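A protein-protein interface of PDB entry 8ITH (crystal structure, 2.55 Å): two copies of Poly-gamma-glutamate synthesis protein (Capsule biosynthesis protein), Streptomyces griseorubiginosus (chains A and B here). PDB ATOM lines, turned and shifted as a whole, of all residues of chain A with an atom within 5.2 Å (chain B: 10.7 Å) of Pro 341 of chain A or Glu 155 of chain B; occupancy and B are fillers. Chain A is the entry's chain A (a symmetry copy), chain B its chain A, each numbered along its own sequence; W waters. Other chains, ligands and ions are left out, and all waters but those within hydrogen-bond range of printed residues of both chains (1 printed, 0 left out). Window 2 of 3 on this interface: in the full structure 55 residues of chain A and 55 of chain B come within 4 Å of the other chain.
Among the printed residues, merely in contact across the chains: Asp 323 of chain A with Glu 155 of chain B (3.2 Å), Arg 324 of chain A with Glu 155 of chain B (3.97 Å), Arg 324 of chain A with Leu 156 of chain B (3.8 Å), Val 325 of chain A with Glu 155 of chain B (3.6 Å), Val 325 of chain A with Leu 156 of chain B (3.9 Å) and Pro 341 of chain A with Glu 155 of chain B (3.7 Å).
Water W1 lies within hydrogen-bond range of the side-chain carboxylate (OE2) of Glu 155 of chain B, the backbone carbonyl oxygen (O) of Leu 339 of chain A and the side-chain hydroxyl (OH) of Tyr 330 of chain A.
Of the 8 printed residues of chain B, 3 touch a printed residue of chain A.
Hydrophobic or aromatic side chains of chain B within 4 Å of the printed part of chain A: Leu 156.
Along chain A the printed residues that touch a printed residue of chain B span positions 323 to 341.
Among the printed residues, 8 pairs touch across the chains.
Asp 323 of chain A touches just one residue of chain B: Glu 155 (3.2 Å).
Arg 324 of chain A touches just these residues of chain B: Glu 155 (3.97 Å) and Leu 156 (3.8 Å).
Val 325 of chain A touches just these residues of chain B: Ser 153, Glu 155 and Leu 156.
Thr 340 of chain A touches none of the printed residues of chain B.
Pro 341 of chain A touches one residue of chain B.
No residue of chain B comes within 4 Å of Tyr 345 of chain A.
Of the printed residues of chain A, Ser 153 of chain B touches Val 325 (2.8 Å).
Printed residues of chain A within 4 Å of Leu 156 of chain B: Arg 324 (3.8 Å) and Val 325 (3.9 Å).
Gly 158 of chain B touches none of the printed residues of chain A.
The nearest printed residue of chain B that does not touch Tyr 330 of chain A is Ser 153 of chain B (4.03 Å).
The side-chain hydroxyl (OG) of Ser 153 of chain B sits at hydrogen-bond distance from the backbone carbonyl oxygen (O) of Val 325 of chain A (2.8 Å).
OH of Tyr 330 of chain A lies within hydrogen-bond range of OE1 of Glu 155 of chain B, 2.8 Å away.
No position is printed for both chains.
Of the 8 pairs that touch across the chains among the printed residues, none has its exchanged pair printed and touching as well.
The backbone NH of Glu 155 of chain B lies close to the side-chain hydroxyl of Ser 153 of chain B (3.2 Å).
The side-chain hydroxyl (OG) of Ser 153 of chain B lies within hydrogen-bond range of the backbone NH (N) of Leu 156 of chain B, at 2.9 Å.
The backbone NH (N) of Arg 324 of chain A is in hydrogen-bond range of the side-chain hydroxyl (OG1) of Thr 322 of chain A.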
ATOM      1  N   THR A 322      -8.621 -29.880 -25.042  1.00  0.00           N
ATOM      2  CA  THR A 322      -9.402 -31.092 -24.844  1.00  0.00           C
ATOM      3  C   THR A 322     -10.859 -30.857 -25.227  1.00  0.00           C
ATOM      4  O   THR A 322     -11.425 -29.791 -24.972  1.00  0.00           O
ATOM      5  CB  THR A 322      -9.306 -31.565 -23.392  1.00  0.00           C
ATOM      6  OG1 THR A 322     -10.146 -32.710 -23.201  1.00  0.00           O
ATOM      7  CG2 THR A 322      -9.748 -30.475 -22.446  1.00  0.00           C
ATOM      8  N   ASP A 323     -11.461 -31.862 -25.862  1.00  0.00           N
ATOM      9  CA  ASP A 323     -12.863 -31.817 -26.248  1.00  0.00           C
ATOM     10  C   ASP A 323     -13.755 -32.571 -25.271  1.00  0.00           C
ATOM     11  O   ASP A 323     -14.898 -32.900 -25.609  1.00  0.00           O
ATOM     12  CB  ASP A 323     -13.045 -32.382 -27.658  1.00  0.00           C
ATOM     13  CG  ASP A 323     -13.784 -31.426 -28.579  1.00  0.00           C
ATOM     14  OD1 ASP A 323     -13.457 -31.385 -29.783  1.00  0.00           O
ATOM     15  OD2 ASP A 323     -14.677 -30.701 -28.093  1.00  0.00           O
ATOM     16  N   ARG A 324     -13.257 -32.861 -24.070  1.00  0.00           N
ATOM     17  CA  ARG A 324     -13.975 -33.652 -23.072  1.00  0.00           C
ATOM     18  C   ARG A 324     -13.955 -32.871 -21.762  1.00  0.00           C
ATOM     19  O   ARG A 324     -13.011 -32.989 -20.975  1.00  0.00           O
ATOM     20  CB  ARG A 324     -13.342 -35.034 -22.917  1.00  0.00           C
ATOM     21  CG  ARG A 324     -13.141 -35.782 -24.227  1.00  0.00           C
ATOM     22  CD  ARG A 324     -14.316 -36.689 -24.546  1.00  0.00           C
ATOM     23  NE  ARG A 324     -14.251 -37.216 -25.906  1.00  0.00           N
ATOM     24  CZ  ARG A 324     -13.468 -38.222 -26.286  1.00  0.00           C
ATOM     25  NH1 ARG A 324     -12.668 -38.815 -25.410  1.00  0.00           N
ATOM     26  NH2 ARG A 324     -13.479 -38.634 -27.547  1.00  0.00           N
ATOM     27  N   VAL A 325     -14.994 -32.073 -21.528  1.00  0.00           N
ATOM     28  CA  VAL A 325     -15.124 -31.274 -20.313  1.00  0.00           C
ATOM     29  C   VAL A 325     -16.335 -31.784 -19.544  1.00  0.00           C
ATOM     30  O   VAL A 325     -17.448 -31.828 -20.082  1.00  0.00           O
ATOM     31  CB  VAL A 325     -15.255 -29.776 -20.628  1.00  0.00           C
ATOM     32  CG1 VAL A 325     -15.520 -28.984 -19.357  1.00  0.00           C
ATOM     33  CG2 VAL A 325     -13.996 -29.271 -21.317  1.00  0.00           C
ATOM     34  N   TYR A 330     -17.477 -27.730 -15.974  1.00  0.00           N
ATOM     35  CA  TYR A 330     -18.225 -26.608 -16.536  1.00  0.00           C
ATOM     36  C   TYR A 330     -18.792 -25.707 -15.448  1.00  0.00           C
ATOM     37  O   TYR A 330     -18.892 -24.489 -15.641  1.00  0.00           O
ATOM     38  CB  TYR A 330     -19.363 -27.112 -17.427  1.00  0.00           C
ATOM     39  CG  TYR A 330     -18.976 -27.407 -18.859  1.00  0.00           C
ATOM     40  CD1 TYR A 330     -18.461 -26.410 -19.681  1.00  0.00           C
ATOM     41  CD2 TYR A 330     -19.152 -28.676 -19.399  1.00  0.00           C
ATOM     42  CE1 TYR A 330     -18.113 -26.675 -20.997  1.00  0.00           C
ATOM     43  CE2 TYR A 330     -18.811 -28.950 -20.712  1.00  0.00           C
ATOM     44  CZ  TYR A 330     -18.291 -27.947 -21.507  1.00  0.00           C
ATOM     45  OH  TYR A 330     -17.949 -28.220 -22.813  1.00  0.00           O
ATOM     46  N   LEU A 339     -21.703 -23.552 -22.587  1.00  0.00           N
ATOM     47  CA  LEU A 339     -20.386 -23.286 -23.142  1.00  0.00           C
ATOM     48  C   LEU A 339     -19.878 -24.467 -23.958  1.00  0.00           C
ATOM     49  O   LEU A 339     -20.179 -25.627 -23.667  1.00  0.00           O
ATOM     50  CB  LEU A 339     -19.380 -22.968 -22.034  1.00  0.00           C
ATOM     51  CG  LEU A 339     -19.552 -21.644 -21.293  1.00  0.00           C
ATOM     52  CD1 LEU A 339     -18.415 -21.432 -20.303  1.00  0.00           C
ATOM     53  CD2 LEU A 339     -19.633 -20.494 -22.279  1.00  0.00           C
ATOM     54  N   THR A 340     -19.110 -24.152 -24.992  1.00  0.00           N
ATOM     55  CA  THR A 340     -18.296 -25.111 -25.718  1.00  0.00           C
ATOM     56  C   THR A 340     -16.945 -25.250 -25.029  1.00  0.00           C
ATOM     57  O   THR A 340     -16.541 -24.371 -24.262  1.00  0.00           O
ATOM     58  CB  THR A 340     -18.117 -24.655 -27.167  1.00  0.00           C
ATOM     59  OG1 THR A 340     -17.487 -23.368 -27.195  1.00  0.00           O
ATOM     60  CG2 THR A 340     -19.464 -24.572 -27.871  1.00  0.00           C
ATOM     61  N   PRO A 341     -16.224 -26.356 -25.259  1.00  0.00           N
ATOM     62  CA  PRO A 341     -14.947 -26.552 -24.544  1.00  0.00           C
ATOM     63  C   PRO A 341     -13.966 -25.398 -24.691  1.00  0.00           C
ATOM     64  O   PRO A 341     -13.384 -24.957 -23.691  1.00  0.00           O
ATOM     65  CB  PRO A 341     -14.405 -27.846 -25.165  1.00  0.00           C
ATOM     66  CG  PRO A 341     -15.619 -28.584 -25.600  1.00  0.00           C
ATOM     67  CD  PRO A 341     -16.591 -27.537 -26.062  1.00  0.00           C
ATOM     68  N   GLY A 342     -13.772 -24.893 -25.912  1.00  0.00           N
ATOM     69  CA  GLY A 342     -12.815 -23.815 -26.113  1.00  0.00           C
ATOM     70  C   GLY A 342     -13.222 -22.526 -25.421  1.00  0.00           C
ATOM     71  O   GLY A 342     -12.382 -21.827 -24.848  1.00  0.00           O
ATOM     72  N   ARG A 343     -14.513 -22.189 -25.475  1.00  0.00           N
ATOM     73  CA  ARG A 343     -15.001 -21.022 -24.748  1.00  0.00           C
ATOM     74  C   ARG A 343     -14.881 -21.211 -23.242  1.00  0.00           C
ATOM     75  O   ARG A 343     -14.636 -20.242 -22.517  1.00  0.00           O
ATOM     76  CB  ARG A 343     -16.451 -20.727 -25.126  1.00  0.00           C
ATOM     77  CG  ARG A 343     -16.643 -20.169 -26.524  1.00  0.00           C
ATOM     78  CD  ARG A 343     -18.108 -19.838 -26.769  1.00  0.00           C
ATOM     79  NE  ARG A 343     -18.333 -19.240 -28.081  1.00  0.00           N
ATOM     80  CZ  ARG A 343     -18.631 -19.932 -29.176  1.00  0.00           C
ATOM     81  NH1 ARG A 343     -18.739 -21.253 -29.121  1.00  0.00           N
ATOM     82  NH2 ARG A 343     -18.821 -19.302 -30.327  1.00  0.00           N
ATOM     83  N   TYR A 344     -15.060 -22.442 -22.756  1.00  0.00           N
ATOM     84  CA  TYR A 344     -14.943 -22.696 -21.323  1.00  0.00           C
ATOM     85  C   TYR A 344     -13.528 -22.427 -20.826  1.00  0.00           C
ATOM     86  O   TYR A 344     -13.340 -21.817 -19.766  1.00  0.00           O
ATOM     87  CB  TYR A 344     -15.361 -24.132 -21.011  1.00  0.00           C
ATOM     88  CG  TYR A 344     -14.720 -24.717 -19.771  1.00  0.00           C
ATOM     89  CD1 TYR A 344     -15.222 -24.435 -18.507  1.00  0.00           C
ATOM     90  CD2 TYR A 344     -13.620 -25.564 -19.868  1.00  0.00           C
ATOM     91  CE1 TYR A 344     -14.641 -24.972 -17.370  1.00  0.00           C
ATOM     92  CE2 TYR A 344     -13.032 -26.108 -18.737  1.00  0.00           C
ATOM     93  CZ  TYR A 344     -13.549 -25.808 -17.491  1.00  0.00           C
ATOM     94  OH  TYR A 344     -12.973 -26.342 -16.360  1.00  0.00           O
ATOM     95  N   TYR A 345     -12.518 -22.869 -21.580  1.00  0.00           N
ATOM     96  CA  TYR A 345     -11.139 -22.640 -21.160  1.00  0.00           C
ATOM     97  C   TYR A 345     -10.748 -21.176 -21.278  1.00  0.00           C
ATOM     98  O   TYR A 345      -9.941 -20.686 -20.480  1.00  0.00           O
ATOM     99  CB  TYR A 345     -10.183 -23.521 -21.969  1.00  0.00           C
ATOM    100  CG  TYR A 345     -10.111 -24.923 -21.424  1.00  0.00           C
ATOM    101  CD1 TYR A 345      -9.387 -25.195 -20.271  1.00  0.00           C
ATOM    102  CD2 TYR A 345     -10.786 -25.972 -22.042  1.00  0.00           C
ATOM    103  CE1 TYR A 345      -9.324 -26.469 -19.752  1.00  0.00           C
ATOM    104  CE2 TYR A 345     -10.731 -27.254 -21.529  1.00  0.00           C
ATOM    105  CZ  TYR A 345      -9.996 -27.494 -20.383  1.00  0.00           C
ATOM    106  OH  TYR A 345      -9.927 -28.761 -19.855  1.00  0.00           O
ATOM    107  N   ASP A 346     -11.308 -20.461 -22.256  1.00  0.00           N
ATOM    108  CA  ASP A 346     -11.016 -19.038 -22.374  1.00  0.00           C
ATOM    109  C   ASP A 346     -11.548 -18.274 -21.169  1.00  0.00           C
ATOM    110  O   ASP A 346     -10.877 -17.377 -20.649  1.00  0.00           O
ATOM    111  CB  ASP A 346     -11.604 -18.485 -23.671  1.00  0.00           C
ATOM    112  CG  ASP A 346     -11.140 -17.071 -23.960  1.00  0.00           C
ATOM    113  OD1 ASP A 346      -9.944 -16.888 -24.269  1.00  0.00           O
ATOM    114  OD2 ASP A 346     -11.969 -16.141 -23.875  1.00  0.00           O
ATOM    115  N   ASP B 151     -24.058 -35.263 -12.911  1.00  0.00           N
ATOM    116  CA  ASP B 151     -24.867 -35.215 -14.117  1.00  0.00           C
ATOM    117  C   ASP B 151     -23.980 -35.159 -15.352  1.00  0.00           C
ATOM    118  O   ASP B 151     -22.808 -34.778 -15.275  1.00  0.00           O
ATOM    119  CB  ASP B 151     -25.797 -34.005 -14.075  1.00  0.00           C
ATOM    120  CG  ASP B 151     -27.150 -34.338 -13.478  1.00  0.00           C
ATOM    121  OD1 ASP B 151     -27.548 -35.523 -13.531  1.00  0.00           O
ATOM    122  OD2 ASP B 151     -27.817 -33.418 -12.960  1.00  0.00           O
ATOM    123  N   PRO B 152     -24.506 -35.548 -16.512  1.00  0.00           N
ATOM    124  CA  PRO B 152     -23.689 -35.530 -17.730  1.00  0.00           C
ATOM    125  C   PRO B 152     -23.461 -34.118 -18.246  1.00  0.00           C
ATOM    126  O   PRO B 152     -24.170 -33.168 -17.906  1.00  0.00           O
ATOM    127  CB  PRO B 152     -24.515 -36.348 -18.733  1.00  0.00           C
ATOM    128  CG  PRO B 152     -25.566 -37.047 -17.918  1.00  0.00           C
ATOM    129  CD  PRO B 152     -25.821 -36.169 -16.741  1.00  0.00           C
ATOM    130  N   SER B 153     -22.441 -33.999 -19.078  1.00  0.00           N
ATOM    131  CA  SER B 153     -22.147 -32.824 -19.878  1.00  0.00           C
ATOM    132  C   SER B 153     -22.413 -33.146 -21.346  1.00  0.00           C
ATOM    133  O   SER B 153     -22.712 -34.293 -21.696  1.00  0.00           O
ATOM    134  CB  SER B 153     -20.687 -32.396 -19.670  1.00  0.00           C
ATOM    135  OG  SER B 153     -19.795 -33.259 -20.356  1.00  0.00           O
ATOM    136  N   PRO B 154     -22.338 -32.153 -22.240  1.00  0.00           N
ATOM    137  CA  PRO B 154     -22.493 -32.466 -23.671  1.00  0.00           C
ATOM    138  C   PRO B 154     -21.438 -33.420 -24.207  1.00  0.00           C
ATOM    139  O   PRO B 154     -21.665 -34.039 -25.253  1.00  0.00           O
ATOM    140  CB  PRO B 154     -22.397 -31.090 -24.343  1.00  0.00           C
ATOM    141  CG  PRO B 154     -22.851 -30.135 -23.297  1.00  0.00           C
ATOM    142  CD  PRO B 154     -22.354 -30.697 -21.998  1.00  0.00           C
ATOM    143  N   GLU B 155     -20.301 -33.572 -23.524  1.00  0.00           N
ATOM    144  CA  GLU B 155     -19.204 -34.388 -24.024  1.00  0.00           C
ATOM    145  C   GLU B 155     -18.855 -35.587 -23.154  1.00  0.00           C
ATOM    146  O   GLU B 155     -18.173 -36.495 -23.642  1.00  0.00           O
ATOM    147  CB  GLU B 155     -17.936 -33.537 -24.196  1.00  0.00           C
ATOM    148  CG  GLU B 155     -18.055 -32.455 -25.248  1.00  0.00           C
ATOM    149  CD  GLU B 155     -18.454 -31.112 -24.673  1.00  0.00           C
ATOM    150  OE1 GLU B 155     -18.215 -30.889 -23.468  1.00  0.00           O
ATOM    151  OE2 GLU B 155     -19.003 -30.279 -25.429  1.00  0.00           O
ATOM    152  N   LEU B 156     -19.280 -35.621 -21.897  1.00  0.00           N
ATOM    153  CA  LEU B 156     -18.936 -36.721 -21.015  1.00  0.00           C
ATOM    154  C   LEU B 156     -20.173 -37.196 -20.270  1.00  0.00           C
ATOM    155  O   LEU B 156     -21.092 -36.411 -20.016  1.00  0.00           O
ATOM    156  CB  LEU B 156     -17.855 -36.307 -20.005  1.00  0.00           C
ATOM    157  CG  LEU B 156     -16.444 -36.121 -20.568  1.00  0.00           C
ATOM    158  CD1 LEU B 156     -15.522 -35.552 -19.503  1.00  0.00           C
ATOM    159  CD2 LEU B 156     -15.901 -37.439 -21.110  1.00  0.00           C
ATOM    160  N   PRO B 157     -20.228 -38.477 -19.912  1.00  0.00           N
ATOM    161  CA  PRO B 157     -21.351 -38.972 -19.111  1.00  0.00           C
ATOM    162  C   PRO B 157     -21.269 -38.450 -17.685  1.00  0.00           C
ATOM    163  O   PRO B 157     -20.282 -37.847 -17.260  1.00  0.00           O
ATOM    164  CB  PRO B 157     -21.174 -40.493 -19.155  1.00  0.00           C
ATOM    165  CG  PRO B 157     -19.698 -40.677 -19.327  1.00  0.00           C
ATOM    166  CD  PRO B 157     -19.258 -39.544 -20.219  1.00  0.00           C
ATOM    167  N   GLY B 158     -22.341 -38.689 -16.939  1.00  0.00           N
ATOM    168  CA  GLY B 158     -22.331 -38.386 -15.528  1.00  0.00           C
ATOM    169  C   GLY B 158     -21.507 -39.414 -14.771  1.00  0.00           C
ATOM    170  O   GLY B 158     -20.736 -40.186 -15.341  1.00  0.00           O
HETATM  171  O   HOH W   1     -20.370 -28.257 -25.115  1.00  0.00           O
